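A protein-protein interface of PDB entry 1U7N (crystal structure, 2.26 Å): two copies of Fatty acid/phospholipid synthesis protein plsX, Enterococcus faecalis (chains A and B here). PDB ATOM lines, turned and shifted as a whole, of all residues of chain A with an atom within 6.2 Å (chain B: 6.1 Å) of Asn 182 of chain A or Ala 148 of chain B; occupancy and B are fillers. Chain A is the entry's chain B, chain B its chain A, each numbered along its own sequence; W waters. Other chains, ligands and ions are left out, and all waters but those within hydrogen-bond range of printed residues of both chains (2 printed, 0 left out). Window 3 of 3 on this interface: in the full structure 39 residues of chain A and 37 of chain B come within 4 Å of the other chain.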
ATOM      1  N   LEU A 180     -27.162  -8.620 -31.081  1.00  0.00           N
ATOM      2  CA  LEU A 180     -26.417  -7.730 -31.967  1.00  0.00           C
ATOM      3  C   LEU A 180     -25.494  -6.875 -31.108  1.00  0.00           C
ATOM      4  O   LEU A 180     -25.956  -6.181 -30.179  1.00  0.00           O
ATOM      5  CB  LEU A 180     -27.356  -6.843 -32.786  1.00  0.00           C
ATOM      6  CG  LEU A 180     -26.716  -5.888 -33.814  1.00  0.00           C
ATOM      7  CD1 LEU A 180     -25.821  -6.644 -34.820  1.00  0.00           C
ATOM      8  CD2 LEU A 180     -27.809  -5.110 -34.544  1.00  0.00           C
ATOM      9  N   ASN A 181     -24.201  -6.935 -31.412  1.00  0.00           N
ATOM     10  CA  ASN A 181     -23.201  -6.257 -30.607  1.00  0.00           C
ATOM     11  C   ASN A 181     -22.106  -5.667 -31.500  1.00  0.00           C
ATOM     12  O   ASN A 181     -22.090  -5.914 -32.700  1.00  0.00           O
ATOM     13  CB  ASN A 181     -22.618  -7.213 -29.553  1.00  0.00           C
ATOM     14  CG  ASN A 181     -22.396  -6.530 -28.200  1.00  0.00           C
ATOM     15  OD1 ASN A 181     -22.088  -5.336 -28.129  1.00  0.00           O
ATOM     16  ND2 ASN A 181     -22.562  -7.290 -27.122  1.00  0.00           N
ATOM     17  N   ASN A 182     -21.210  -4.888 -30.912  1.00  0.00           N
ATOM     18  CA  ASN A 182     -20.113  -4.236 -31.649  1.00  0.00           C
ATOM     19  C   ASN A 182     -18.852  -5.085 -31.802  1.00  0.00           C
ATOM     20  O   ASN A 182     -17.845  -4.624 -32.337  1.00  0.00           O
ATOM     21  CB  ASN A 182     -19.782  -2.872 -31.025  1.00  0.00           C
ATOM     22  CG  ASN A 182     -19.381  -2.968 -29.559  1.00  0.00           C
ATOM     23  OD1 ASN A 182     -19.394  -4.044 -28.959  1.00  0.00           O
ATOM     24  ND2 ASN A 182     -19.016  -1.831 -28.975  1.00  0.00           N
ATOM     25  N   GLY A 183     -18.926  -6.325 -31.332  1.00  0.00           N
ATOM     26  CA  GLY A 183     -17.838  -7.299 -31.437  1.00  0.00           C
ATOM     27  C   GLY A 183     -18.302  -8.626 -30.863  1.00  0.00           C
ATOM     28  O   GLY A 183     -19.436  -8.729 -30.415  1.00  0.00           O
ATOM     29  N   THR A 184     -17.432  -9.637 -30.874  1.00  0.00           N
ATOM     30  CA  THR A 184     -17.802 -10.999 -30.437  1.00  0.00           C
ATOM     31  C   THR A 184     -17.594 -11.270 -28.945  1.00  0.00           C
ATOM     32  O   THR A 184     -18.304 -12.105 -28.362  1.00  0.00           O
ATOM     33  CB  THR A 184     -17.048 -12.101 -31.221  1.00  0.00           C
ATOM     34  OG1 THR A 184     -15.685 -11.700 -31.431  1.00  0.00           O
ATOM     35  CG2 THR A 184     -17.719 -12.372 -32.561  1.00  0.00           C
ATOM     36  N   LYS A 188     -16.966  -5.410 -23.945  1.00  0.00           N
ATOM     37  CA  LYS A 188     -17.477  -5.728 -25.296  1.00  0.00           C
ATOM     38  C   LYS A 188     -18.948  -5.350 -25.452  1.00  0.00           C
ATOM     39  O   LYS A 188     -19.857  -6.157 -25.193  1.00  0.00           O
ATOM     40  CB  LYS A 188     -17.110  -7.096 -25.879  1.00  0.00           C
ATOM     41  CG  LYS A 188     -17.185  -7.139 -27.434  1.00  0.00           C
ATOM     42  CD  LYS A 188     -16.718  -5.847 -28.119  1.00  0.00           C
ATOM     43  CE  LYS A 188     -15.194  -5.735 -28.221  1.00  0.00           C
ATOM     44  NZ  LYS A 188     -14.721  -5.985 -29.619  1.00  0.00           N
ATOM     45  N   GLY A 189     -19.164  -4.097 -25.836  1.00  0.00           N
ATOM     46  CA  GLY A 189     -20.504  -3.575 -25.952  1.00  0.00           C
ATOM     47  C   GLY A 189     -20.746  -2.269 -25.235  1.00  0.00           C
ATOM     48  O   GLY A 189     -19.896  -1.772 -24.496  1.00  0.00           O
ATOM     49  N   SER A 190     -21.923  -1.713 -25.476  1.00  0.00           N
ATOM     50  CA  SER A 190     -22.363  -0.530 -24.781  1.00  0.00           C
ATOM     51  C   SER A 190     -22.816  -0.939 -23.372  1.00  0.00           C
ATOM     52  O   SER A 190     -22.806  -2.128 -23.033  1.00  0.00           O
ATOM     53  CB  SER A 190     -23.487   0.138 -25.571  1.00  0.00           C
ATOM     54  OG  SER A 190     -24.615  -0.702 -25.677  1.00  0.00           O
ATOM     55  N   GLU A 191     -23.192   0.019 -22.536  1.00  0.00           N
ATOM     56  CA  GLU A 191     -23.762  -0.333 -21.231  1.00  0.00           C
ATOM     57  C   GLU A 191     -24.978  -1.245 -21.412  1.00  0.00           C
ATOM     58  O   GLU A 191     -25.100  -2.258 -20.721  1.00  0.00           O
ATOM     59  CB  GLU A 191     -24.137   0.911 -20.425  1.00  0.00           C
ATOM     60  CG  GLU A 191     -22.956   1.629 -19.778  1.00  0.00           C
ATOM     61  CD  GLU A 191     -23.309   3.036 -19.336  1.00  0.00           C
ATOM     62  OE1 GLU A 191     -22.408   3.906 -19.356  1.00  0.00           O
ATOM     63  OE2 GLU A 191     -24.490   3.279 -18.985  1.00  0.00           O
ATOM     64  N   THR A 193     -25.733  -3.357 -24.001  1.00  0.00           N
ATOM     65  CA  THR A 193     -25.438  -4.723 -24.477  1.00  0.00           C
ATOM     66  C   THR A 193     -24.536  -5.532 -23.554  1.00  0.00           C
ATOM     67  O   THR A 193     -24.593  -6.754 -23.569  1.00  0.00           O
ATOM     68  CB  THR A 193     -24.939  -4.808 -25.950  1.00  0.00           C
ATOM     69  OG1 THR A 193     -23.662  -4.167 -26.079  1.00  0.00           O
ATOM     70  CG2 THR A 193     -25.975  -4.199 -26.919  1.00  0.00           C
ATOM     71  N   VAL A 212     -23.647 -11.535 -31.978  1.00  0.00           N
ATOM     72  CA  VAL A 212     -23.580 -11.559 -33.434  1.00  0.00           C
ATOM     73  C   VAL A 212     -23.205 -10.179 -33.958  1.00  0.00           C
ATOM     74  O   VAL A 212     -23.605  -9.152 -33.403  1.00  0.00           O
ATOM     75  CB  VAL A 212     -24.878 -12.100 -34.112  1.00  0.00           C
ATOM     76  CG1 VAL A 212     -25.150 -13.557 -33.683  1.00  0.00           C
ATOM     77  CG2 VAL A 212     -26.063 -11.204 -33.843  1.00  0.00           C
ATOM     78  N   GLU A 213     -22.425 -10.182 -35.028  1.00  0.00           N
ATOM     79  CA  GLU A 213     -21.949  -8.978 -35.665  1.00  0.00           C
ATOM     80  C   GLU A 213     -22.761  -8.637 -36.897  1.00  0.00           C
ATOM     81  O   GLU A 213     -23.200  -9.518 -37.635  1.00  0.00           O
ATOM     82  CB  GLU A 213     -20.475  -9.137 -36.012  1.00  0.00           C
ATOM     83  CG  GLU A 213     -19.604  -9.331 -34.780  1.00  0.00           C
ATOM     84  CD  GLU A 213     -18.155  -9.454 -35.107  1.00  0.00           C
ATOM     85  OE1 GLU A 213     -17.732 -10.516 -35.618  1.00  0.00           O
ATOM     86  OE2 GLU A 213     -17.433  -8.471 -34.860  1.00  0.00           O
ATOM     87  N   ARG B 122     -14.241  12.838 -26.029  1.00  0.00           N
ATOM     88  CA  ARG B 122     -14.340  11.604 -26.833  1.00  0.00           C
ATOM     89  C   ARG B 122     -13.960  11.774 -28.305  1.00  0.00           C
ATOM     90  O   ARG B 122     -14.763  12.239 -29.116  1.00  0.00           O
ATOM     91  CB  ARG B 122     -15.744  10.987 -26.736  1.00  0.00           C
ATOM     92  CG  ARG B 122     -16.236  10.795 -25.308  1.00  0.00           C
ATOM     93  CD  ARG B 122     -15.729   9.505 -24.655  1.00  0.00           C
ATOM     94  NE  ARG B 122     -16.692   8.996 -23.669  1.00  0.00           N
ATOM     95  CZ  ARG B 122     -17.887   8.472 -23.979  1.00  0.00           C
ATOM     96  NH1 ARG B 122     -18.286   8.402 -25.247  1.00  0.00           N
ATOM     97  NH2 ARG B 122     -18.704   8.025 -23.029  1.00  0.00           N
ATOM     98  N   ASP B 143     -19.279   8.873 -34.902  1.00  0.00           N
ATOM     99  CA  ASP B 143     -18.279   7.882 -34.536  1.00  0.00           C
ATOM    100  C   ASP B 143     -18.600   6.537 -35.161  1.00  0.00           C
ATOM    101  O   ASP B 143     -19.703   6.035 -35.013  1.00  0.00           O
ATOM    102  CB  ASP B 143     -18.284   7.759 -33.003  1.00  0.00           C
ATOM    103  CG  ASP B 143     -17.187   6.853 -32.460  1.00  0.00           C
ATOM    104  OD1 ASP B 143     -17.293   6.513 -31.267  1.00  0.00           O
ATOM    105  OD2 ASP B 143     -16.217   6.511 -33.194  1.00  0.00           O
ATOM    106  N   GLY B 145     -16.862   3.818 -34.276  1.00  0.00           N
ATOM    107  CA  GLY B 145     -16.590   2.781 -33.275  1.00  0.00           C
ATOM    108  C   GLY B 145     -15.529   3.032 -32.211  1.00  0.00           C
ATOM    109  O   GLY B 145     -15.169   2.115 -31.503  1.00  0.00           O
ATOM    110  N   ALA B 146     -14.995   4.244 -32.100  1.00  0.00           N
ATOM    111  CA  ALA B 146     -14.116   4.563 -30.974  1.00  0.00           C
ATOM    112  C   ALA B 146     -14.842   4.317 -29.628  1.00  0.00           C
ATOM    113  O   ALA B 146     -14.246   3.819 -28.679  1.00  0.00           O
ATOM    114  CB  ALA B 146     -13.630   5.994 -31.060  1.00  0.00           C
ATOM    115  N   ASN B 147     -16.129   4.664 -29.566  1.00  0.00           N
ATOM    116  CA  ASN B 147     -16.894   4.619 -28.324  1.00  0.00           C
ATOM    117  C   ASN B 147     -18.101   3.700 -28.452  1.00  0.00           C
ATOM    118  O   ASN B 147     -18.643   3.541 -29.532  1.00  0.00           O
ATOM    119  CB  ASN B 147     -17.351   6.031 -27.947  1.00  0.00           C
ATOM    120  CG  ASN B 147     -16.194   7.015 -27.850  1.00  0.00           C
ATOM    121  OD1 ASN B 147     -15.439   6.978 -26.883  1.00  0.00           O
ATOM    122  ND2 ASN B 147     -16.051   7.907 -28.857  1.00  0.00           N
ATOM    123  N   ALA B 148     -18.519   3.075 -27.373  1.00  0.00           N
ATOM    124  CA  ALA B 148     -19.704   2.237 -27.419  1.00  0.00           C
ATOM    125  C   ALA B 148     -20.884   2.980 -26.795  1.00  0.00           C
ATOM    126  O   ALA B 148     -22.036   2.594 -26.991  1.00  0.00           O
ATOM    127  CB  ALA B 148     -19.449   0.922 -26.707  1.00  0.00           C
ATOM    128  N   ASP B 149     -20.577   4.061 -26.072  1.00  0.00           N
ATOM    129  CA  ASP B 149     -21.576   4.955 -25.489  1.00  0.00           C
ATOM    130  C   ASP B 149     -21.226   6.407 -25.742  1.00  0.00           C
ATOM    131  O   ASP B 149     -20.052   6.782 -25.683  1.00  0.00           O
ATOM    132  CB  ASP B 149     -21.674   4.706 -23.982  1.00  0.00           C
ATOM    133  CG  ASP B 149     -22.489   3.467 -23.662  1.00  0.00           C
ATOM    134  OD1 ASP B 149     -23.725   3.547 -23.743  1.00  0.00           O
ATOM    135  OD2 ASP B 149     -21.905   2.415 -23.344  1.00  0.00           O
ATOM    136  N   ASN B 150     -22.230   7.240 -26.024  1.00  0.00           N
ATOM    137  CA  ASN B 150     -21.969   8.651 -26.230  1.00  0.00           C
ATOM    138  C   ASN B 150     -23.022   9.472 -25.520  1.00  0.00           C
ATOM    139  O   ASN B 150     -24.102   8.964 -25.197  1.00  0.00           O
ATOM    140  CB  ASN B 150     -21.878   9.011 -27.738  1.00  0.00           C
ATOM    141  CG  ASN B 150     -20.485   8.745 -28.336  1.00  0.00           C
ATOM    142  OD1 ASN B 150     -19.473   9.300 -27.887  1.00  0.00           O
ATOM    143  ND2 ASN B 150     -20.431   7.899 -29.332  1.00  0.00           N
ATOM    144  N   ASP B 228     -23.482   8.208 -32.615  1.00  0.00           N
ATOM    145  CA  ASP B 228     -22.716   7.543 -31.579  1.00  0.00           C
ATOM    146  C   ASP B 228     -21.978   6.302 -32.126  1.00  0.00           C
ATOM    147  O   ASP B 228     -22.430   5.652 -33.087  1.00  0.00           O
ATOM    148  CB  ASP B 228     -23.645   7.105 -30.441  1.00  0.00           C
ATOM    149  CG  ASP B 228     -24.543   5.957 -30.846  1.00  0.00           C
ATOM    150  OD1 ASP B 228     -25.577   6.226 -31.492  1.00  0.00           O
ATOM    151  OD2 ASP B 228     -24.204   4.791 -30.534  1.00  0.00           O
ATOM    152  N   GLY B 229     -20.863   5.969 -31.480  1.00  0.00           N
ATOM    153  CA  GLY B 229     -20.012   4.871 -31.896  1.00  0.00           C
ATOM    154  C   GLY B 229     -20.600   3.486 -32.043  1.00  0.00           C
ATOM    155  O   GLY B 229     -20.127   2.704 -32.879  1.00  0.00           O
ATOM    156  N   PHE B 230     -21.615   3.162 -31.246  1.00  0.00           N
ATOM    157  CA  PHE B 230     -22.307   1.874 -31.390  1.00  0.00           C
ATOM    158  C   PHE B 230     -23.200   1.781 -32.653  1.00  0.00           C
ATOM    159  O   PHE B 230     -23.141   0.802 -33.410  1.00  0.00           O
ATOM    160  CB  PHE B 230     -23.133   1.564 -30.145  1.00  0.00           C
ATOM    161  CG  PHE B 230     -23.634   0.153 -30.109  1.00  0.00           C
ATOM    162  CD1 PHE B 230     -22.854  -0.865 -29.526  1.00  0.00           C
ATOM    163  CD2 PHE B 230     -24.865  -0.177 -30.683  1.00  0.00           C
ATOM    164  CE1 PHE B 230     -23.311  -2.193 -29.498  1.00  0.00           C
ATOM    165  CE2 PHE B 230     -25.330  -1.497 -30.665  1.00  0.00           C
ATOM    166  CZ  PHE B 230     -24.543  -2.513 -30.066  1.00  0.00           C
ATOM    167  N   ASN B 233     -20.853   1.990 -35.781  1.00  0.00           N
ATOM    168  CA  ASN B 233     -20.260   0.681 -36.053  1.00  0.00           C
ATOM    169  C   ASN B 233     -21.278  -0.238 -36.740  1.00  0.00           C
ATOM    170  O   ASN B 233     -20.960  -0.878 -37.737  1.00  0.00           O
ATOM    171  CB  ASN B 233     -19.723   0.035 -34.758  1.00  0.00           C
ATOM    172  CG  ASN B 233     -19.233  -1.406 -34.958  1.00  0.00           C
ATOM    173  OD1 ASN B 233     -18.156  -1.632 -35.472  1.00  0.00           O
ATOM    174  ND2 ASN B 233     -20.034  -2.379 -34.532  1.00  0.00           N
ATOM    175  N   LYS B 237     -20.916  -1.578 -40.682  1.00  0.00           N
ATOM    176  CA  LYS B 237     -20.758  -3.009 -40.972  1.00  0.00           C
ATOM    177  C   LYS B 237     -21.968  -3.660 -41.650  1.00  0.00           C
ATOM    178  O   LYS B 237     -21.807  -4.628 -42.388  1.00  0.00           O
ATOM    179  CB  LYS B 237     -20.223  -3.790 -39.763  1.00  0.00           C
ATOM    180  CG  LYS B 237     -21.167  -3.929 -38.626  1.00  0.00           C
ATOM    181  CD  LYS B 237     -20.413  -4.394 -37.342  1.00  0.00           C
ATOM    182  CE  LYS B 237     -21.441  -4.744 -36.214  1.00  0.00           C
ATOM    183  NZ  LYS B 237     -20.933  -5.663 -35.177  1.00  0.00           N
HETATM  184  O   HOH W   1     -18.916   0.446 -30.891  1.00  0.00           O
HETATM  185  O   HOH W   2     -23.337  -3.906 -33.931  1.00  0.00           O
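Among the printed residues, merely in contact across the chains: Ser 190 of chain A with Ala 148 of chain B, Ser 190 of chain A with Asp 149 of chain B, Asn 182 of chain A with Asn 233 of chain B, Glu 213 of chain A with Lys 237 of chain B, Gly 189 of chain A with Ala 148 of chain B, Asn 182 of chain A with Ala 148 of chain B, Asn 181 of chain A with Phe 230 of chain B, Asn 182 of chain A with Phe 230 of chain B, Thr 193 of chain A with Phe 230 of chain B, Asn 182 of chain A with Lys 237 of chain B and Leu 180 of chain A with Phe 230 of chain B.
Water W2 bridges O of Asn 181 of chain A (2.7 Å) and NZ of Lys 237 of chain B (3.2 Å). Water W1 lies within hydrogen-bond range of the side-chain amide nitrogen (ND2) of Asn 182 of chain A, the backbone carbonyl oxygen (O) of Gly 229 of chain B and the backbone carbonyl oxygen (O) of Asn 147 of chain B.
Of the printed residues of chain B, Asn 182 of chain A touches Ala 148 (3.6 Å), Phe 230 (3.7 Å), Asn 233 (3.4 Å) and Lys 237 (3.9 Å). Of the printed residues of chain A, Ala 148 of chain B touches Asn 182 (3.6 Å), Gly 189 (3.5 Å) and Ser 190 (3.2 Å). Printed residues of chain B within 4 Å of Glu 213 of chain A: Lys 237. Printed residues of chain A within 4 Å of Phe 230 of chain B: Leu 180 (3.9 Å), Asn 181 (3.6 Å), Asn 182 (3.7 Å) and Thr 193 (3.8 Å). Of the printed residues of chain B, Glu 191 of chain A touches Asp 149 (2.8 Å).
NH1 of Arg 122 of chain B lies within hydrogen-bond range of O of Asp 149 of chain B, at 2.4 Å. The backbone carbonyl oxygen (O) of Asn 147 of chain B is in hydrogen-bond range of the backbone NH (N) of Phe 230 of chain B (3.5 Å). The side-chain carboxylate (OD2) of Asp 228 of chain B sits at hydrogen-bond distance from the backbone NH (N) of Phe 230 of chain B (3.1 Å). The side-chain amide oxygen (OD1) of Asn 181 of chain A sits close to the side-chain amide oxygen (OD1) of Asn 182 of chain A (3.1 Å). O of Val 212 of chain A is in hydrogen-bond range of N of Asn 181 of chain A, 3.0 Å away. OG1 of Thr 193 of chain A is in hydrogen-bond range of N of Ser 190 of chain A, at 3.1 Å.
Of the 12 printed residues of chain A, 8 touch a printed residue of chain B. Among the printed residues, no Asp or Glu carboxylate lies within 4 Å of a Lys or Arg side-chain nitrogen of the other chain.
N of Glu 191 of chain A sits at hydrogen-bond distance from OD2 of Asp 149 of chain B (2.8 Å). O of Asn 181 of chain A is in hydrogen-bond range of NZ of Lys 237 of chain B (2.7 Å).
No position is printed for both chains. Of the 13 pairs that touch across the chains among the printed residues, none has its exchanged pair printed and touching as well.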
